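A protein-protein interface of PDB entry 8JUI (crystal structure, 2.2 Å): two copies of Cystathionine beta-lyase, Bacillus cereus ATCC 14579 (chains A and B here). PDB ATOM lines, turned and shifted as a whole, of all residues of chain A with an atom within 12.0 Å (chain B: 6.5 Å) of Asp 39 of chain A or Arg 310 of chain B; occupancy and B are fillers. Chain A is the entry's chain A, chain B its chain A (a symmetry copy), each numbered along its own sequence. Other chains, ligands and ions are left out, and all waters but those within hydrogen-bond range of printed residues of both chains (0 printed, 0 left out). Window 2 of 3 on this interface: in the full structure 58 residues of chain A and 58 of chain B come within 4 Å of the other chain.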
ATOM      1  N   PHE A  33      28.824 -10.031   1.713  1.00  0.00           N
ATOM      2  CA  PHE A  33      28.763  -8.562   1.963  1.00  0.00           C
ATOM      3  C   PHE A  33      28.586  -8.275   3.468  1.00  0.00           C
ATOM      4  O   PHE A  33      27.601  -8.763   4.092  1.00  0.00           O
ATOM      5  CB  PHE A  33      27.653  -7.940   1.112  1.00  0.00           C
ATOM      6  CG  PHE A  33      27.830  -8.099  -0.379  1.00  0.00           C
ATOM      7  CD1 PHE A  33      27.377  -9.237  -1.036  1.00  0.00           C
ATOM      8  CD2 PHE A  33      28.418  -7.095  -1.132  1.00  0.00           C
ATOM      9  CE1 PHE A  33      27.542  -9.386  -2.404  1.00  0.00           C
ATOM     10  CE2 PHE A  33      28.556  -7.233  -2.510  1.00  0.00           C
ATOM     11  CZ  PHE A  33      28.138  -8.385  -3.137  1.00  0.00           C
ATOM     12  N   HIS A  34      29.504  -7.503   4.062  1.00  0.00           N
ATOM     13  CA  HIS A  34      29.396  -6.995   5.463  1.00  0.00           C
ATOM     14  C   HIS A  34      28.074  -6.210   5.616  1.00  0.00           C
ATOM     15  O   HIS A  34      27.748  -5.432   4.734  1.00  0.00           O
ATOM     16  CB  HIS A  34      30.619  -6.159   5.868  1.00  0.00           C
ATOM     17  CG  HIS A  34      30.524  -5.577   7.243  1.00  0.00           C
ATOM     18  ND1 HIS A  34      30.761  -6.335   8.393  1.00  0.00           N
ATOM     19  CD2 HIS A  34      30.248  -4.313   7.664  1.00  0.00           C
ATOM     20  CE1 HIS A  34      30.635  -5.578   9.464  1.00  0.00           C
ATOM     21  NE2 HIS A  34      30.317  -4.329   9.036  1.00  0.00           N
ATOM     22  N   GLN A  35      27.328  -6.461   6.688  1.00  0.00           N
ATOM     23  CA  GLN A  35      26.082  -5.729   7.060  1.00  0.00           C
ATOM     24  C   GLN A  35      26.479  -4.676   8.106  1.00  0.00           C
ATOM     25  O   GLN A  35      26.942  -5.084   9.195  1.00  0.00           O
ATOM     26  CB  GLN A  35      25.039  -6.710   7.617  1.00  0.00           C
ATOM     27  CG  GLN A  35      23.974  -7.143   6.621  1.00  0.00           C
ATOM     28  CD  GLN A  35      24.534  -7.820   5.392  1.00  0.00           C
ATOM     29  OE1 GLN A  35      25.266  -8.799   5.501  1.00  0.00           O
ATOM     30  NE2 GLN A  35      24.182  -7.320   4.212  1.00  0.00           N
ATOM     31  N   PHE A  36      26.344  -3.385   7.785  1.00  0.00           N
ATOM     32  CA  PHE A  36      26.708  -2.257   8.690  1.00  0.00           C
ATOM     33  C   PHE A  36      25.637  -2.066   9.794  1.00  0.00           C
ATOM     34  O   PHE A  36      25.931  -1.329  10.757  1.00  0.00           O
ATOM     35  CB  PHE A  36      26.988  -0.993   7.862  1.00  0.00           C
ATOM     36  CG  PHE A  36      28.275  -1.003   7.060  1.00  0.00           C
ATOM     37  CD1 PHE A  36      29.489  -0.675   7.647  1.00  0.00           C
ATOM     38  CD2 PHE A  36      28.271  -1.311   5.703  1.00  0.00           C
ATOM     39  CE1 PHE A  36      30.667  -0.674   6.901  1.00  0.00           C
ATOM     40  CE2 PHE A  36      29.446  -1.302   4.956  1.00  0.00           C
ATOM     41  CZ  PHE A  36      30.646  -0.985   5.554  1.00  0.00           C
ATOM     42  N   ASP A  37      24.463  -2.709   9.684  1.00  0.00           N
ATOM     43  CA  ASP A  37      23.333  -2.647  10.659  1.00  0.00           C
ATOM     44  C   ASP A  37      22.880  -4.072  11.034  1.00  0.00           C
ATOM     45  O   ASP A  37      22.939  -4.966  10.162  1.00  0.00           O
ATOM     46  CB  ASP A  37      22.158  -1.840  10.091  1.00  0.00           C
ATOM     47  CG  ASP A  37      21.002  -1.656  11.071  1.00  0.00           C
ATOM     48  OD1 ASP A  37      21.222  -1.011  12.113  1.00  0.00           O
ATOM     49  OD2 ASP A  37      19.891  -2.180  10.799  1.00  0.00           O
ATOM     50  N   VAL A  38      22.407  -4.275  12.271  1.00  0.00           N
ATOM     51  CA  VAL A  38      21.930  -5.603  12.783  1.00  0.00           C
ATOM     52  C   VAL A  38      20.584  -5.980  12.141  1.00  0.00           C
ATOM     53  O   VAL A  38      20.398  -7.190  11.849  1.00  0.00           O
ATOM     54  CB  VAL A  38      21.841  -5.629  14.321  1.00  0.00           C
ATOM     55  CG1 VAL A  38      21.196  -6.909  14.829  1.00  0.00           C
ATOM     56  CG2 VAL A  38      23.205  -5.427  14.960  1.00  0.00           C
ATOM     57  N   ASP A  39      19.703  -4.988  11.915  1.00  0.00           N
ATOM     58  CA  ASP A  39      18.268  -5.184  11.558  1.00  0.00           C
ATOM     59  C   ASP A  39      18.062  -5.104  10.036  1.00  0.00           C
ATOM     60  O   ASP A  39      17.650  -6.138   9.465  1.00  0.00           O
ATOM     61  CB  ASP A  39      17.391  -4.245  12.389  1.00  0.00           C
ATOM     62  CG  ASP A  39      17.497  -4.577  13.871  1.00  0.00           C
ATOM     63  OD1 ASP A  39      17.201  -5.733  14.250  1.00  0.00           O
ATOM     64  OD2 ASP A  39      17.954  -3.718  14.623  1.00  0.00           O
ATOM     65  N   THR A  40      18.343  -3.960   9.402  1.00  0.00           N
ATOM     66  CA  THR A  40      18.342  -3.779   7.914  1.00  0.00           C
ATOM     67  C   THR A  40      19.689  -4.232   7.309  1.00  0.00           C
ATOM     68  O   THR A  40      20.728  -4.075   7.991  1.00  0.00           O
ATOM     69  CB  THR A  40      18.046  -2.325   7.526  1.00  0.00           C
ATOM     70  OG1 THR A  40      18.784  -1.517   8.446  1.00  0.00           O
ATOM     71  CG2 THR A  40      16.567  -1.991   7.550  1.00  0.00           C
ATOM     72  N   PHE A  41      19.679  -4.726   6.063  1.00  0.00           N
ATOM     73  CA  PHE A  41      20.711  -5.653   5.523  1.00  0.00           C
ATOM     74  C   PHE A  41      21.684  -4.965   4.548  1.00  0.00           C
ATOM     75  O   PHE A  41      22.844  -5.459   4.460  1.00  0.00           O
ATOM     76  CB  PHE A  41      20.035  -6.902   4.943  1.00  0.00           C
ATOM     77  CG  PHE A  41      19.979  -8.057   5.918  1.00  0.00           C
ATOM     78  CD1 PHE A  41      19.538  -7.866   7.224  1.00  0.00           C
ATOM     79  CD2 PHE A  41      20.399  -9.330   5.546  1.00  0.00           C
ATOM     80  CE1 PHE A  41      19.509  -8.917   8.130  1.00  0.00           C
ATOM     81  CE2 PHE A  41      20.358 -10.381   6.450  1.00  0.00           C
ATOM     82  CZ  PHE A  41      19.913 -10.171   7.737  1.00  0.00           C
ATOM     83  N   GLY A  42      21.287  -3.866   3.891  1.00  0.00           N
ATOM     84  CA  GLY A  42      22.070  -3.248   2.796  1.00  0.00           C
ATOM     85  C   GLY A  42      21.643  -3.808   1.441  1.00  0.00           C
ATOM     86  O   GLY A  42      20.986  -4.879   1.403  1.00  0.00           O
ATOM     87  N   LYS A  43      21.970  -3.137   0.338  1.00  0.00           N
ATOM     88  CA  LYS A  43      21.477  -3.568  -1.006  1.00  0.00           C
ATOM     89  C   LYS A  43      21.817  -5.052  -1.294  1.00  0.00           C
ATOM     90  O   LYS A  43      20.997  -5.740  -1.923  1.00  0.00           O
ATOM     91  CB  LYS A  43      22.020  -2.668  -2.119  1.00  0.00           C
ATOM     92  CG  LYS A  43      21.593  -3.130  -3.498  1.00  0.00           C
ATOM     93  CD  LYS A  43      21.438  -2.041  -4.519  1.00  0.00           C
ATOM     94  CE  LYS A  43      20.632  -2.547  -5.697  1.00  0.00           C
ATOM     95  NZ  LYS A  43      20.732  -1.649  -6.869  1.00  0.00           N
ATOM     96  N   TYR A  44      22.966  -5.545  -0.826  1.00  0.00           N
ATOM     97  CA  TYR A  44      23.499  -6.906  -1.110  1.00  0.00           C
ATOM     98  C   TYR A  44      23.822  -7.620   0.206  1.00  0.00           C
ATOM     99  O   TYR A  44      24.402  -6.969   1.124  1.00  0.00           O
ATOM    100  CB  TYR A  44      24.713  -6.778  -2.039  1.00  0.00           C
ATOM    101  CG  TYR A  44      24.439  -5.968  -3.282  1.00  0.00           C
ATOM    102  CD1 TYR A  44      23.704  -6.503  -4.331  1.00  0.00           C
ATOM    103  CD2 TYR A  44      24.900  -4.663  -3.407  1.00  0.00           C
ATOM    104  CE1 TYR A  44      23.466  -5.776  -5.485  1.00  0.00           C
ATOM    105  CE2 TYR A  44      24.650  -3.913  -4.546  1.00  0.00           C
ATOM    106  CZ  TYR A  44      23.934  -4.478  -5.591  1.00  0.00           C
ATOM    107  OH  TYR A  44      23.659  -3.748  -6.714  1.00  0.00           O
ATOM    108  N   ASP A  45      23.386  -8.883   0.314  1.00  0.00           N
ATOM    109  CA  ASP A  45      23.642  -9.794   1.460  1.00  0.00           C
ATOM    110  C   ASP A  45      24.566 -10.929   0.979  1.00  0.00           C
ATOM    111  O   ASP A  45      25.412 -11.410   1.791  1.00  0.00           O
ATOM    112  CB  ASP A  45      22.321 -10.271   2.081  1.00  0.00           C
ATOM    113  CG  ASP A  45      21.630 -11.448   1.399  1.00  0.00           C
ATOM    114  OD1 ASP A  45      21.433 -11.393   0.158  1.00  0.00           O
ATOM    115  OD2 ASP A  45      21.278 -12.418   2.119  1.00  0.00           O
ATOM    116  N   LEU B 303      24.584 -15.442  24.453  1.00  0.00           N
ATOM    117  CA  LEU B 303      24.690 -14.488  25.578  1.00  0.00           C
ATOM    118  C   LEU B 303      23.436 -14.601  26.466  1.00  0.00           C
ATOM    119  O   LEU B 303      22.595 -15.546  26.248  1.00  0.00           O
ATOM    120  CB  LEU B 303      24.937 -13.107  24.977  1.00  0.00           C
ATOM    121  CG  LEU B 303      26.306 -12.995  24.308  1.00  0.00           C
ATOM    122  CD1 LEU B 303      26.526 -11.629  23.716  1.00  0.00           C
ATOM    123  CD2 LEU B 303      27.418 -13.322  25.286  1.00  0.00           C
ATOM    124  N   SER B 305      21.011 -12.430  27.055  1.00  0.00           N
ATOM    125  CA  SER B 305      19.794 -11.839  26.458  1.00  0.00           C
ATOM    126  C   SER B 305      20.118 -11.282  25.070  1.00  0.00           C
ATOM    127  O   SER B 305      21.329 -11.123  24.744  1.00  0.00           O
ATOM    128  CB  SER B 305      19.279 -10.736  27.360  1.00  0.00           C
ATOM    129  OG  SER B 305      20.255  -9.707  27.508  1.00  0.00           O
ATOM    130  N   GLU B 306      19.070 -10.954  24.310  1.00  0.00           N
ATOM    131  CA  GLU B 306      19.149 -10.243  23.011  1.00  0.00           C
ATOM    132  C   GLU B 306      19.843  -8.891  23.210  1.00  0.00           C
ATOM    133  O   GLU B 306      20.329  -8.293  22.227  1.00  0.00           O
ATOM    134  CB  GLU B 306      17.743 -10.074  22.444  1.00  0.00           C
ATOM    135  CG  GLU B 306      17.708  -9.137  21.258  1.00  0.00           C
ATOM    136  CD  GLU B 306      16.451  -9.233  20.428  1.00  0.00           C
ATOM    137  OE1 GLU B 306      15.582 -10.046  20.778  1.00  0.00           O
ATOM    138  OE2 GLU B 306      16.361  -8.501  19.431  1.00  0.00           O
ATOM    139  N   ASP B 307      19.858  -8.424  24.453  1.00  0.00           N
ATOM    140  CA  ASP B 307      20.330  -7.073  24.828  1.00  0.00           C
ATOM    141  C   ASP B 307      21.850  -7.117  24.893  1.00  0.00           C
ATOM    142  O   ASP B 307      22.508  -6.203  24.354  1.00  0.00           O
ATOM    143  CB  ASP B 307      19.728  -6.643  26.169  1.00  0.00           C
ATOM    144  CG  ASP B 307      19.318  -5.191  26.141  1.00  0.00           C
ATOM    145  OD1 ASP B 307      18.386  -4.880  25.371  1.00  0.00           O
ATOM    146  OD2 ASP B 307      19.974  -4.383  26.826  1.00  0.00           O
ATOM    147  N   ALA B 308      22.360  -8.133  25.583  1.00  0.00           N
ATOM    148  CA  ALA B 308      23.796  -8.453  25.695  1.00  0.00           C
ATOM    149  C   ALA B 308      24.343  -8.672  24.273  1.00  0.00           C
ATOM    150  O   ALA B 308      25.330  -8.004  23.904  1.00  0.00           O
ATOM    151  CB  ALA B 308      23.953  -9.655  26.592  1.00  0.00           C
ATOM    152  N   LEU B 309      23.642  -9.473  23.469  1.00  0.00           N
ATOM    153  CA  LEU B 309      24.062  -9.857  22.096  1.00  0.00           C
ATOM    154  C   LEU B 309      24.262  -8.576  21.281  1.00  0.00           C
ATOM    155  O   LEU B 309      25.339  -8.453  20.641  1.00  0.00           O
ATOM    156  CB  LEU B 309      23.042 -10.823  21.469  1.00  0.00           C
ATOM    157  CG  LEU B 309      23.258 -11.169  19.987  1.00  0.00           C
ATOM    158  CD1 LEU B 309      22.622 -12.491  19.621  1.00  0.00           C
ATOM    159  CD2 LEU B 309      22.727 -10.080  19.055  1.00  0.00           C
ATOM    160  N   ARG B 310      23.309  -7.637  21.347  1.00  0.00           N
ATOM    161  CA  ARG B 310      23.344  -6.357  20.580  1.00  0.00           C
ATOM    162  C   ARG B 310      24.463  -5.473  21.124  1.00  0.00           C
ATOM    163  O   ARG B 310      25.081  -4.725  20.316  1.00  0.00           O
ATOM    164  CB  ARG B 310      21.999  -5.618  20.631  1.00  0.00           C
ATOM    165  CG  ARG B 310      20.868  -6.378  19.953  1.00  0.00           C
ATOM    166  CD  ARG B 310      19.494  -5.762  20.136  1.00  0.00           C
ATOM    167  NE  ARG B 310      19.098  -5.331  18.812  1.00  0.00           N
ATOM    168  CZ  ARG B 310      18.357  -6.031  17.976  1.00  0.00           C
ATOM    169  NH1 ARG B 310      17.837  -7.187  18.351  1.00  0.00           N
ATOM    170  NH2 ARG B 310      18.111  -5.556  16.770  1.00  0.00           N
ATOM    171  N   LYS B 311      24.740  -5.567  22.425  1.00  0.00           N
ATOM    172  CA  LYS B 311      25.834  -4.774  23.037  1.00  0.00           C
ATOM    173  C   LYS B 311      27.171  -5.318  22.518  1.00  0.00           C
ATOM    174  O   LYS B 311      27.996  -4.516  22.038  1.00  0.00           O
ATOM    175  CB  LYS B 311      25.784  -4.819  24.566  1.00  0.00           C
ATOM    176  CG  LYS B 311      26.921  -4.074  25.252  1.00  0.00           C
ATOM    177  CD  LYS B 311      27.129  -2.661  24.745  1.00  0.00           C
ATOM    178  CE  LYS B 311      25.950  -1.745  25.025  1.00  0.00           C
ATOM    179  NZ  LYS B 311      26.401  -0.366  25.307  1.00  0.00           N
ATOM    180  N   PHE B 312      27.348  -6.637  22.617  1.00  0.00           N
ATOM    181  CA  PHE B 312      28.525  -7.384  22.112  1.00  0.00           C
ATOM    182  C   PHE B 312      28.769  -6.970  20.646  1.00  0.00           C
ATOM    183  O   PHE B 312      29.863  -6.497  20.346  1.00  0.00           O
ATOM    184  CB  PHE B 312      28.298  -8.872  22.365  1.00  0.00           C
ATOM    185  CG  PHE B 312      29.398  -9.768  21.861  1.00  0.00           C
ATOM    186  CD1 PHE B 312      29.359 -10.292  20.577  1.00  0.00           C
ATOM    187  CD2 PHE B 312      30.477 -10.081  22.670  1.00  0.00           C
ATOM    188  CE1 PHE B 312      30.378 -11.116  20.120  1.00  0.00           C
ATOM    189  CE2 PHE B 312      31.492 -10.907  22.212  1.00  0.00           C
ATOM    190  CZ  PHE B 312      31.439 -11.421  20.937  1.00  0.00           C
ATOM    191  N   LEU B 313      27.757  -7.044  19.775  1.00  0.00           N
ATOM    192  CA  LEU B 313      27.920  -6.744  18.325  1.00  0.00           C
ATOM    193  C   LEU B 313      28.384  -5.300  18.139  1.00  0.00           C
ATOM    194  O   LEU B 313      29.223  -5.054  17.250  1.00  0.00           O
ATOM    195  CB  LEU B 313      26.614  -7.006  17.569  1.00  0.00           C
ATOM    196  CG  LEU B 313      26.292  -8.487  17.339  1.00  0.00           C
ATOM    197  CD1 LEU B 313      24.972  -8.645  16.602  1.00  0.00           C
ATOM    198  CD2 LEU B 313      27.411  -9.199  16.571  1.00  0.00           C
ATOM    199  N   SER B 314      27.865  -4.380  18.950  1.00  0.00           N
ATOM    200  CA  SER B 314      28.193  -2.934  18.864  1.00  0.00           C
ATOM    201  C   SER B 314      29.661  -2.697  19.234  1.00  0.00           C
ATOM    202  O   SER B 314      30.176  -1.692  18.762  1.00  0.00           O
ATOM    203  CB  SER B 314      27.259  -2.102  19.739  1.00  0.00           C
ATOM    204  OG  SER B 314      27.522  -2.340  21.119  1.00  0.00           O
ATOM    205  N   LYS B 315      30.293  -3.556  20.052  1.00  0.00           N
ATOM    206  CA  LYS B 315      31.678  -3.358  20.596  1.00  0.00           C
ATOM    207  C   LYS B 315      32.769  -4.179  19.858  1.00  0.00           C
ATOM    208  O   LYS B 315      33.904  -3.677  19.790  1.00  0.00           O
ATOM    209  CB  LYS B 315      31.738  -3.731  22.081  1.00  0.00           C
ATOM    210  CG  LYS B 315      30.845  -2.892  22.987  1.00  0.00           C
ATOM    211  CD  LYS B 315      31.406  -1.521  23.320  1.00  0.00           C
ATOM    212  CE  LYS B 315      30.886  -0.399  22.455  1.00  0.00           C
ATOM    213  NZ  LYS B 315      31.001   0.903  23.163  1.00  0.00           N
ATOM    214  N   PHE B 321      30.481  -8.870   9.811  1.00  0.00           N
ATOM    215  CA  PHE B 321      29.079  -9.214  10.176  1.00  0.00           C
ATOM    216  C   PHE B 321      28.328  -9.499   8.885  1.00  0.00           C
ATOM    217  O   PHE B 321      28.059  -8.590   8.104  1.00  0.00           O
ATOM    218  CB  PHE B 321      28.436  -8.126  11.050  1.00  0.00           C
ATOM    219  CG  PHE B 321      27.049  -8.474  11.536  1.00  0.00           C
ATOM    220  CD1 PHE B 321      26.848  -9.511  12.435  1.00  0.00           C
ATOM    221  CD2 PHE B 321      25.934  -7.771  11.099  1.00  0.00           C
ATOM    222  CE1 PHE B 321      25.572  -9.860  12.864  1.00  0.00           C
ATOM    223  CE2 PHE B 321      24.657  -8.115  11.532  1.00  0.00           C
ATOM    224  CZ  PHE B 321      24.473  -9.162  12.414  1.00  0.00           C
ATOM    225  N   TYR B 334      24.046 -13.648  12.949  1.00  0.00           N
ATOM    226  CA  TYR B 334      22.892 -13.628  13.880  1.00  0.00           C
ATOM    227  C   TYR B 334      21.816 -14.483  13.241  1.00  0.00           C
ATOM    228  O   TYR B 334      21.030 -13.996  12.444  1.00  0.00           O
ATOM    229  CB  TYR B 334      22.457 -12.180  14.101  1.00  0.00           C
ATOM    230  CG  TYR B 334      21.535 -11.914  15.265  1.00  0.00           C
ATOM    231  CD1 TYR B 334      21.022 -12.926  16.075  1.00  0.00           C
ATOM    232  CD2 TYR B 334      21.135 -10.615  15.529  1.00  0.00           C
ATOM    233  CE1 TYR B 334      20.174 -12.641  17.133  1.00  0.00           C
ATOM    234  CE2 TYR B 334      20.288 -10.317  16.589  1.00  0.00           C
ATOM    235  CZ  TYR B 334      19.792 -11.328  17.387  1.00  0.00           C
ATOM    236  OH  TYR B 334      18.949 -10.996  18.415  1.00  0.00           O
ATOM    237  N   LYS B 337      18.107 -13.445  12.900  1.00  0.00           N
ATOM    238  CA  LYS B 337      17.911 -12.314  11.936  1.00  0.00           C
ATOM    239  C   LYS B 337      18.397 -12.587  10.507  1.00  0.00           C
ATOM    240  O   LYS B 337      18.123 -11.748   9.639  1.00  0.00           O
ATOM    241  CB  LYS B 337      18.618 -11.049  12.416  1.00  0.00           C
ATOM    242  CG  LYS B 337      18.098 -10.486  13.730  1.00  0.00           C
ATOM    243  CD  LYS B 337      16.752  -9.811  13.614  1.00  0.00           C
ATOM    244  CE  LYS B 337      16.204  -9.379  14.957  1.00  0.00           C
ATOM    245  NZ  LYS B 337      16.250 -10.505  15.918  1.00  0.00           N
ATOM    246  N   ASN B 355      17.190 -15.604  20.248  1.00  0.00           N
ATOM    247  CA  ASN B 355      17.590 -14.215  19.892  1.00  0.00           C
ATOM    248  C   ASN B 355      18.837 -13.765  20.666  1.00  0.00           C
ATOM    249  O   ASN B 355      19.282 -12.629  20.435  1.00  0.00           O
ATOM    250  CB  ASN B 355      16.432 -13.263  20.169  1.00  0.00           C
ATOM    251  CG  ASN B 355      15.323 -13.345  19.143  1.00  0.00           C
ATOM    252  OD1 ASN B 355      14.601 -12.369  18.982  1.00  0.00           O
ATOM    253  ND2 ASN B 355      15.185 -14.461  18.438  1.00  0.00           N
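Hydrophobic or aromatic side chains of chain A that line the printed part of chain B: His 34, Val 38 and Phe 41.
Among the printed residues, 9 pairs touch across the chains.
Among the printed residues, Asp or Glu carboxylates within 4 Å of a Lys or Arg side-chain nitrogen of the other chain: Asp 39 of chain A with Arg 310 of chain B.
No position is printed for both chains.
Of chain B, only Arg 310 (2.7 Å) and Lys 337 (3.8 Å) come within 4 Å of Asp 39 of chain A.
Arg 310 of chain B touches just these residues of chain A: Val 38 (3.9 Å) and Asp 39 (2.7 Å).
No residue of chain A comes within 4 Å of Ser 305 of chain B.
No residue of chain A comes within 4 Å of Glu 306 of chain B.
No residue of chain A comes within 4 Å of Ala 308 of chain B.
Of chain A, only Asp 39 (3.8 Å) and Phe 41 (3.1 Å) come within 4 Å of Lys 337 of chain B.
Of the printed residues of chain A, Phe 321 of chain B touches His 34, Gln 35, Asp 37 and Val 38.
Of the printed residues of chain B, Asp 37 of chain A touches Phe 321 (3.8 Å).
Of the printed residues of chain B, Val 38 of chain A touches Arg 310, Phe 321 and Tyr 334.
The nearest residue of chain B that does not touch Asp 39 of chain A is Phe 321 of chain B (5.9 Å).
The nearest residue of chain A that does not touch Arg 310 of chain B is Asp 37 of chain A (7.1 Å).
The nearest printed residue of chain B that does not touch Val 38 of chain A is Leu 313 of chain B (4.02 Å).
OG1 of Thr 40 of chain A sits at hydrogen-bond distance from OD2 of Asp 37 of chain A (2.7 Å).
The backbone carbonyl oxygen (O) of Asn 355 of chain B lies within hydrogen-bond range of the side-chain hydroxyl (OH) of Tyr 334 of chain B.
The side-chain carboxylate (OD2) of Asp 37 of chain A is in hydrogen-bond range of the backbone NH (N) of Asp 39 of chain A, at 3.0 Å.
NE2 of Gln 35 of chain A sits at hydrogen-bond distance from O of Tyr 44 of chain A, at 3.1 Å.
OE1 of Gln 35 of chain A sits close to O of Phe 33 of chain A, at 2.7 Å.
Among the printed residues, merely in contact across the chains: Phe 41 of chain A with Lys 337 of chain B (3.1 Å), Val 38 of chain A with Tyr 334 of chain B (3.8 Å), Asp 37 of chain A with Phe 321 of chain B (3.8 Å), Asp 39 of chain A with Lys 337 of chain B (3.8 Å), Val 38 of chain A with Arg 310 of chain B (3.9 Å) and Val 38 of chain A with Phe 321 of chain B (3.9 Å).
OD1 of Asp 39 of chain A is in salt-bridge range of NH2 of Arg 310 of chain B.
A ring nitrogen (ND1) of His 34 of chain A is in hydrogen-bond range of the backbone NH (N) of Phe 321 of chain B, at 2.9 Å.
N of Gln 35 of chain A lies within hydrogen-bond range of O of Phe 321 of chain B, 2.7 Å away.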
